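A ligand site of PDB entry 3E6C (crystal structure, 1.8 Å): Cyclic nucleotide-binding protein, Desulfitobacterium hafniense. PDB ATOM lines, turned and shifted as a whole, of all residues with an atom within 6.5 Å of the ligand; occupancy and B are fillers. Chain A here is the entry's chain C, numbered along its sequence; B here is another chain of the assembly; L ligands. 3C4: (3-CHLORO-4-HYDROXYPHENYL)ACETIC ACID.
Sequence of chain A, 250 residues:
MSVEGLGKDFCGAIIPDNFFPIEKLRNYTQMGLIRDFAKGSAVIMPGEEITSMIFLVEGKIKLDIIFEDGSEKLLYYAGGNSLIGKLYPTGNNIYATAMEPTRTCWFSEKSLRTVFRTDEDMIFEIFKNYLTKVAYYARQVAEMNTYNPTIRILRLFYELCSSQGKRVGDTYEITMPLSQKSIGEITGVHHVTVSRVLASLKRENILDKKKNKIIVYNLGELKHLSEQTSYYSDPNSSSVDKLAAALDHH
NZ of Lys 133 lies within hydrogen-bond range of O of Leu 83 (2.7 Å). OG1 of Thr 90 sits at hydrogen-bond distance from N of Asn 92 (3.1 Å). O of Gly 85 is in hydrogen-bond range of OH of Tyr 130 of chain A (2.8 Å). The backbone carbonyl oxygen of Tyr 76 sits at hydrogen-bond distance from the backbone NH of Leu 63, 2.9 Å away. The backbone carbonyl oxygen of Leu 63 sits at hydrogen-bond distance from the backbone NH of Leu 75. The side-chain amide oxygen of Asn 129 is in hydrogen-bond range of the side-chain amino group of Lys 133 (3.1 Å). The backbone carbonyl oxygen (O) of Ala 135 of chain B lies within hydrogen-bond range of the side-chain amide nitrogen (ND2) of Asn 92 (3.2 Å).
Merely in contact with the ligand: Ile 84 (3.4 Å), Tyr 130 of chain A (3.5 Å), Val 134 of chain B (3.6 Å), Leu 131 of chain B (3.6 Å), Ile 94 (3.7 Å), Ala 135 of chain B (3.7 Å), Leu 83 (3.8 Å) and Leu 63 (3.9 Å). Hydrophobic or aromatic side chains that line the ligand: Leu 63, Tyr 76, Ile 84, Ile 94, Tyr 130 of chain A, Leu 131 of chain B, Val 134 of chain B and Ala 135 of chain B. Of the 24 residues printed, 14 come within 4 Å of the ligand. The nearest printed residue that does not touch the ligand is Leu 75 (4.6 Å).
The side-chain hydroxyl (OG1) of Thr 90 lies within hydrogen-bond range of an oxygen (O2) of the ligand, at 2.7 Å. An oxygen (OH) of the ligand sits at hydrogen-bond distance from the side-chain amino group (NZ) of Lys 133 (2.7 Å). An oxygen (O2) of the ligand lies within hydrogen-bond range of the side-chain amide nitrogen (ND2) of Asn 92 (3.0 Å). The backbone NH of Gly 85 sits at hydrogen-bond distance from an oxygen (OH) of the ligand, at 3.0 Å. The side-chain hydroxyl of Tyr 76 sits at hydrogen-bond distance from an oxygen (OH) of the ligand, 2.6 Å away. NZ of Lys 86 is in salt-bridge range of O1 of the ligand, 2.7 Å away.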
ATOM      1  N   LEU A  63      16.069  16.017  10.647  1.00  0.00           N
ATOM      2  CA  LEU A  63      16.860  17.211  10.316  1.00  0.00           C
ATOM      3  C   LEU A  63      16.770  17.553   8.781  1.00  0.00           C
ATOM      4  O   LEU A  63      17.099  16.720   7.901  1.00  0.00           O
ATOM      5  CB  LEU A  63      18.342  16.994  10.772  1.00  0.00           C
ATOM      6  CG  LEU A  63      19.250  18.173  10.606  1.00  0.00           C
ATOM      7  CD1 LEU A  63      20.126  18.366  11.900  1.00  0.00           C
ATOM      8  CD2 LEU A  63      20.107  18.223   9.296  1.00  0.00           C
ATOM      9  N   ILE A  65      16.906  20.703   5.462  1.00  0.00           N
ATOM     10  CA  ILE A  65      17.398  21.983   4.986  1.00  0.00           C
ATOM     11  C   ILE A  65      16.216  22.744   4.367  1.00  0.00           C
ATOM     12  O   ILE A  65      15.360  22.150   3.774  1.00  0.00           O
ATOM     13  CB  ILE A  65      18.498  21.781   3.929  1.00  0.00           C
ATOM     14  CG1 ILE A  65      19.122  23.117   3.525  1.00  0.00           C
ATOM     15  CG2 ILE A  65      17.973  20.962   2.728  1.00  0.00           C
ATOM     16  CD1 ILE A  65      20.549  22.789   2.735  1.00  0.00           C
ATOM     17  N   LEU A  75      17.528  16.043   5.245  1.00  0.00           N
ATOM     18  CA  LEU A  75      18.927  15.641   5.276  1.00  0.00           C
ATOM     19  C   LEU A  75      19.146  14.267   5.925  1.00  0.00           C
ATOM     20  O   LEU A  75      19.702  13.360   5.296  1.00  0.00           O
ATOM     21  CB  LEU A  75      19.797  16.743   5.851  1.00  0.00           C
ATOM     22  CG  LEU A  75      19.939  18.073   5.070  1.00  0.00           C
ATOM     23  CD1 LEU A  75      20.999  19.017   5.652  1.00  0.00           C
ATOM     24  CD2 LEU A  75      20.158  17.866   3.576  1.00  0.00           C
ATOM     25  N   TYR A  76      18.754  14.113   7.182  1.00  0.00           N
ATOM     26  CA  TYR A  76      18.861  12.871   7.853  1.00  0.00           C
ATOM     27  C   TYR A  76      17.980  12.724   9.064  1.00  0.00           C
ATOM     28  O   TYR A  76      17.405  13.684   9.527  1.00  0.00           O
ATOM     29  CB  TYR A  76      20.310  12.631   8.273  1.00  0.00           C
ATOM     30  CG  TYR A  76      20.979  13.579   9.291  1.00  0.00           C
ATOM     31  CD1 TYR A  76      22.064  14.389   8.936  1.00  0.00           C
ATOM     32  CD2 TYR A  76      20.649  13.525  10.629  1.00  0.00           C
ATOM     33  CE1 TYR A  76      22.718  15.091   9.836  1.00  0.00           C
ATOM     34  CE2 TYR A  76      21.308  14.252  11.561  1.00  0.00           C
ATOM     35  CZ  TYR A  76      22.353  15.029  11.164  1.00  0.00           C
ATOM     36  OH  TYR A  76      23.072  15.694  12.081  1.00  0.00           O
ATOM     37  N   LEU A  83      25.179  12.394  16.694  1.00  0.00           N
ATOM     38  CA  LEU A  83      25.865  13.683  16.826  1.00  0.00           C
ATOM     39  C   LEU A  83      25.532  14.582  15.613  1.00  0.00           C
ATOM     40  O   LEU A  83      25.674  14.202  14.444  1.00  0.00           O
ATOM     41  CB  LEU A  83      27.359  13.512  17.003  1.00  0.00           C
ATOM     42  CG  LEU A  83      28.147  14.761  17.375  1.00  0.00           C
ATOM     43  CD1 LEU A  83      27.958  15.096  18.810  1.00  0.00           C
ATOM     44  CD2 LEU A  83      29.688  14.486  16.998  1.00  0.00           C
ATOM     45  N   ILE A  84      24.917  15.732  15.914  1.00  0.00           N
ATOM     46  CA  ILE A  84      24.813  16.924  15.042  1.00  0.00           C
ATOM     47  C   ILE A  84      26.023  17.815  15.138  1.00  0.00           C
ATOM     48  O   ILE A  84      26.291  18.414  16.140  1.00  0.00           O
ATOM     49  CB  ILE A  84      23.497  17.768  15.335  1.00  0.00           C
ATOM     50  CG1 ILE A  84      22.278  16.818  15.352  1.00  0.00           C
ATOM     51  CG2 ILE A  84      23.331  18.806  14.211  1.00  0.00           C
ATOM     52  CD1 ILE A  84      20.840  17.420  15.849  1.00  0.00           C
ATOM     53  N   GLY A  85      26.835  17.832  14.055  1.00  0.00           N
ATOM     54  CA  GLY A  85      28.179  18.418  14.051  1.00  0.00           C
ATOM     55  C   GLY A  85      28.220  19.874  13.638  1.00  0.00           C
ATOM     56  O   GLY A  85      29.259  20.382  13.232  1.00  0.00           O
ATOM     57  N   LYS A  86      27.166  20.632  13.992  1.00  0.00           N
ATOM     58  CA  LYS A  86      27.081  22.098  13.648  1.00  0.00           C
ATOM     59  C   LYS A  86      27.802  23.089  14.547  1.00  0.00           C
ATOM     60  O   LYS A  86      27.230  24.068  15.057  1.00  0.00           O
ATOM     61  CB  LYS A  86      25.602  22.440  13.356  1.00  0.00           C
ATOM     62  CG  LYS A  86      25.069  21.706  12.165  1.00  0.00           C
ATOM     63  CD  LYS A  86      23.563  21.987  11.860  1.00  0.00           C
ATOM     64  CE  LYS A  86      23.152  23.415  11.830  1.00  0.00           C
ATOM     65  NZ  LYS A  86      23.963  24.375  10.939  1.00  0.00           N
ATOM     66  N   TYR A  88      30.002  25.352  13.945  1.00  0.00           N
ATOM     67  CA  TYR A  88      30.335  26.594  13.266  1.00  0.00           C
ATOM     68  C   TYR A  88      29.247  26.855  12.256  1.00  0.00           C
ATOM     69  O   TYR A  88      28.608  25.893  11.770  1.00  0.00           O
ATOM     70  CB  TYR A  88      31.713  26.498  12.530  1.00  0.00           C
ATOM     71  CG  TYR A  88      32.823  26.089  13.487  1.00  0.00           C
ATOM     72  CD1 TYR A  88      33.300  26.983  14.404  1.00  0.00           C
ATOM     73  CD2 TYR A  88      33.345  24.809  13.508  1.00  0.00           C
ATOM     74  CE1 TYR A  88      34.241  26.656  15.342  1.00  0.00           C
ATOM     75  CE2 TYR A  88      34.302  24.452  14.463  1.00  0.00           C
ATOM     76  CZ  TYR A  88      34.735  25.378  15.359  1.00  0.00           C
ATOM     77  OH  TYR A  88      35.661  25.090  16.331  1.00  0.00           O
ATOM     78  N   THR A  90      27.408  27.476   8.700  1.00  0.00           N
ATOM     79  CA  THR A  90      27.611  26.792   7.436  1.00  0.00           C
ATOM     80  C   THR A  90      27.030  27.435   6.208  1.00  0.00           C
ATOM     81  O   THR A  90      27.330  27.017   5.062  1.00  0.00           O
ATOM     82  CB  THR A  90      27.092  25.409   7.464  1.00  0.00           C
ATOM     83  OG1 THR A  90      25.662  25.443   7.477  1.00  0.00           O
ATOM     84  CG2 THR A  90      27.694  24.631   8.701  1.00  0.00           C
ATOM     85  N   GLY A  91      26.173  28.393   6.408  1.00  0.00           N
ATOM     86  CA  GLY A  91      25.480  28.901   5.252  1.00  0.00           C
ATOM     87  C   GLY A  91      24.174  28.207   4.934  1.00  0.00           C
ATOM     88  O   GLY A  91      23.408  28.714   4.148  1.00  0.00           O
ATOM     89  N   ASN A  92      23.896  27.039   5.502  1.00  0.00           N
ATOM     90  CA  ASN A  92      22.639  26.389   5.180  1.00  0.00           C
ATOM     91  C   ASN A  92      21.592  26.709   6.248  1.00  0.00           C
ATOM     92  O   ASN A  92      21.880  26.718   7.451  1.00  0.00           O
ATOM     93  CB  ASN A  92      22.802  24.889   5.091  1.00  0.00           C
ATOM     94  CG  ASN A  92      23.676  24.456   3.900  1.00  0.00           C
ATOM     95  OD1 ASN A  92      23.487  24.962   2.827  1.00  0.00           O
ATOM     96  ND2 ASN A  92      24.517  23.418   4.072  1.00  0.00           N
ATOM     97  N   ASN A  93      20.364  26.894   5.804  1.00  0.00           N
ATOM     98  CA  ASN A  93      19.248  27.018   6.766  1.00  0.00           C
ATOM     99  C   ASN A  93      18.684  25.657   7.191  1.00  0.00           C
ATOM    100  O   ASN A  93      18.044  24.960   6.430  1.00  0.00           O
ATOM    101  CB  ASN A  93      18.154  27.848   6.138  1.00  0.00           C
ATOM    102  CG  ASN A  93      17.028  28.219   7.148  1.00  0.00           C
ATOM    103  OD1 ASN A  93      17.171  27.927   8.337  1.00  0.00           O
ATOM    104  ND2 ASN A  93      15.905  28.806   6.676  1.00  0.00           N
ATOM    105  N   ILE A  94      18.933  25.275   8.421  1.00  0.00           N
ATOM    106  CA  ILE A  94      18.607  23.943   8.901  1.00  0.00           C
ATOM    107  C   ILE A  94      17.367  24.068   9.832  1.00  0.00           C
ATOM    108  O   ILE A  94      17.279  25.017  10.581  1.00  0.00           O
ATOM    109  CB  ILE A  94      19.826  23.377   9.651  1.00  0.00           C
ATOM    110  CG1 ILE A  94      20.997  23.212   8.676  1.00  0.00           C
ATOM    111  CG2 ILE A  94      19.511  21.985  10.254  1.00  0.00           C
ATOM    112  CD1 ILE A  94      20.699  22.322   7.535  1.00  0.00           C
ATOM    113  N   ASN A 129      32.611  10.189  12.761  1.00  0.00           N
ATOM    114  CA  ASN A 129      31.240  10.630  12.579  1.00  0.00           C
ATOM    115  C   ASN A 129      31.150  11.627  11.349  1.00  0.00           C
ATOM    116  O   ASN A 129      30.303  11.500  10.468  1.00  0.00           O
ATOM    117  CB  ASN A 129      30.723  11.250  13.873  1.00  0.00           C
ATOM    118  CG  ASN A 129      29.289  11.756  13.719  1.00  0.00           C
ATOM    119  OD1 ASN A 129      29.092  12.887  13.314  1.00  0.00           O
ATOM    120  ND2 ASN A 129      28.304  10.898  14.003  1.00  0.00           N
ATOM    121  N   TYR A 130      32.047  12.617  11.310  1.00  0.00           N
ATOM    122  CA  TYR A 130      32.075  13.478  10.154  1.00  0.00           C
ATOM    123  C   TYR A 130      32.378  12.733   8.858  1.00  0.00           C
ATOM    124  O   TYR A 130      31.833  13.049   7.770  1.00  0.00           O
ATOM    125  CB  TYR A 130      33.155  14.547  10.282  1.00  0.00           C
ATOM    126  CG  TYR A 130      32.739  15.787  11.028  1.00  0.00           C
ATOM    127  CD1 TYR A 130      33.408  16.174  12.172  1.00  0.00           C
ATOM    128  CD2 TYR A 130      31.690  16.612  10.566  1.00  0.00           C
ATOM    129  CE1 TYR A 130      33.044  17.344  12.859  1.00  0.00           C
ATOM    130  CE2 TYR A 130      31.342  17.851  11.248  1.00  0.00           C
ATOM    131  CZ  TYR A 130      32.001  18.145  12.433  1.00  0.00           C
ATOM    132  OH  TYR A 130      31.792  19.308  13.142  1.00  0.00           O
ATOM    133  N   LYS A 133      29.539  10.993   7.317  1.00  0.00           N
ATOM    134  CA  LYS A 133      28.600  11.855   6.644  1.00  0.00           C
ATOM    135  C   LYS A 133      29.104  12.317   5.301  1.00  0.00           C
ATOM    136  O   LYS A 133      28.390  12.347   4.317  1.00  0.00           O
ATOM    137  CB  LYS A 133      28.380  13.068   7.545  1.00  0.00           C
ATOM    138  CG  LYS A 133      27.542  12.680   8.770  1.00  0.00           C
ATOM    139  CD  LYS A 133      27.405  13.922   9.669  1.00  0.00           C
ATOM    140  CE  LYS A 133      26.732  13.541  11.045  1.00  0.00           C
ATOM    141  NZ  LYS A 133      26.825  14.632  12.072  1.00  0.00           N
ATOM    142  N   CYS B  11      31.739  27.905   7.299  1.00  0.00           N
ATOM    143  CA  CYS B  11      32.092  26.619   6.694  1.00  0.00           C
ATOM    144  C   CYS B  11      31.213  26.394   5.443  1.00  0.00           C
ATOM    145  O   CYS B  11      30.335  25.518   5.395  1.00  0.00           O
ATOM    146  CB  CYS B  11      31.952  25.470   7.721  1.00  0.00           C
ATOM    147  SG  CYS B  11      33.145  25.682   9.075  1.00  0.00           S
ATOM    148  N   TYR B 130      35.977  19.236   7.731  1.00  0.00           N
ATOM    149  CA  TYR B 130      34.935  18.254   7.553  1.00  0.00           C
ATOM    150  C   TYR B 130      33.547  18.871   7.418  1.00  0.00           C
ATOM    151  O   TYR B 130      32.680  18.388   6.647  1.00  0.00           O
ATOM    152  CB  TYR B 130      34.856  17.304   8.743  1.00  0.00           C
ATOM    153  CG  TYR B 130      35.791  16.125   8.681  1.00  0.00           C
ATOM    154  CD1 TYR B 130      36.738  15.929   9.665  1.00  0.00           C
ATOM    155  CD2 TYR B 130      35.706  15.166   7.648  1.00  0.00           C
ATOM    156  CE1 TYR B 130      37.597  14.818   9.630  1.00  0.00           C
ATOM    157  CE2 TYR B 130      36.561  13.987   7.634  1.00  0.00           C
ATOM    158  CZ  TYR B 130      37.542  13.888   8.610  1.00  0.00           C
ATOM    159  OH  TYR B 130      38.378  12.798   8.727  1.00  0.00           O
ATOM    160  N   LEU B 131      33.261  19.792   8.358  1.00  0.00           N
ATOM    161  CA  LEU B 131      31.906  20.441   8.309  1.00  0.00           C
ATOM    162  C   LEU B 131      31.596  21.070   6.990  1.00  0.00           C
ATOM    163  O   LEU B 131      30.463  20.987   6.448  1.00  0.00           O
ATOM    164  CB  LEU B 131      31.765  21.449   9.483  1.00  0.00           C
ATOM    165  CG  LEU B 131      30.430  22.164   9.627  1.00  0.00           C
ATOM    166  CD1 LEU B 131      29.207  21.172   9.638  1.00  0.00           C
ATOM    167  CD2 LEU B 131      30.407  23.013  10.865  1.00  0.00           C
ATOM    168  N   VAL B 134      30.629  18.344   4.545  1.00  0.00           N
ATOM    169  CA  VAL B 134      29.296  17.826   4.798  1.00  0.00           C
ATOM    170  C   VAL B 134      28.233  18.846   4.381  1.00  0.00           C
ATOM    171  O   VAL B 134      27.291  18.475   3.707  1.00  0.00           O
ATOM    172  CB  VAL B 134      29.052  17.449   6.289  1.00  0.00           C
ATOM    173  CG1 VAL B 134      27.576  16.955   6.459  1.00  0.00           C
ATOM    174  CG2 VAL B 134      30.110  16.424   6.786  1.00  0.00           C
ATOM    175  N   ALA B 135      28.380  20.128   4.733  1.00  0.00           N
ATOM    176  CA  ALA B 135      27.439  21.177   4.334  1.00  0.00           C
ATOM    177  C   ALA B 135      27.282  21.277   2.782  1.00  0.00           C
ATOM    178  O   ALA B 135      26.174  21.475   2.221  1.00  0.00           O
ATOM    179  CB  ALA B 135      27.873  22.534   5.015  1.00  0.00           C
ATOM    180  N   TYR B 136      28.420  21.104   2.060  1.00  0.00           N
ATOM    181  CA  TYR B 136      28.417  21.147   0.585  1.00  0.00           C
ATOM    182  C   TYR B 136      27.640  20.044   0.016  1.00  0.00           C
ATOM    183  O   TYR B 136      26.727  20.291  -0.786  1.00  0.00           O
ATOM    184  CB  TYR B 136      29.878  21.224  -0.053  1.00  0.00           C
ATOM    185  CG  TYR B 136      29.785  21.205  -1.541  1.00  0.00           C
ATOM    186  CD1 TYR B 136      29.551  22.377  -2.237  1.00  0.00           C
ATOM    187  CD2 TYR B 136      29.766  19.991  -2.248  1.00  0.00           C
ATOM    188  CE1 TYR B 136      29.295  22.328  -3.624  1.00  0.00           C
ATOM    189  CE2 TYR B 136      29.562  19.929  -3.611  1.00  0.00           C
ATOM    190  CZ  TYR B 136      29.345  21.119  -4.308  1.00  0.00           C
ATOM    191  OH  TYR B 136      29.072  21.151  -5.715  1.00  0.00           O
ATOM    192  N   ALA B 138      25.711  17.638   1.457  1.00  0.00           N
ATOM    193  CA  ALA B 138      24.334  17.534   1.908  1.00  0.00           C
ATOM    194  C   ALA B 138      23.406  18.509   1.190  1.00  0.00           C
ATOM    195  O   ALA B 138      22.339  18.106   0.740  1.00  0.00           O
ATOM    196  CB  ALA B 138      24.246  17.579   3.556  1.00  0.00           C
HETATM  197  O2  3C4 L   1      24.757  22.934   6.992  1.00  0.00           O
HETATM  198  C   3C4 L   1      24.690  22.104   7.910  1.00  0.00           C
HETATM  199  O1  3C4 L   1      24.569  22.468   9.115  1.00  0.00           O
HETATM  200  CG  3C4 L   1      24.944  20.630   7.536  1.00  0.00           C
HETATM  201  CA  3C4 L   1      25.081  19.658   8.613  1.00  0.00           C
HETATM  202  CD2 3C4 L   1      23.923  19.192   9.258  1.00  0.00           C
HETATM  203  CE2 3C4 L   1      23.970  18.369  10.189  1.00  0.00           C
HETATM  204  CZ  3C4 L   1      25.238  17.781  10.703  1.00  0.00           C
HETATM  205  OH  3C4 L   1      25.347  16.829  11.699  1.00  0.00           O
HETATM  206 CL   3C4 L   1      27.903  17.635  10.404  1.00  0.00          CL
HETATM  207  CE1 3C4 L   1      26.398  18.261   9.917  1.00  0.00           C
HETATM  208  CD1 3C4 L   1      26.285  19.133   8.981  1.00  0.00           C
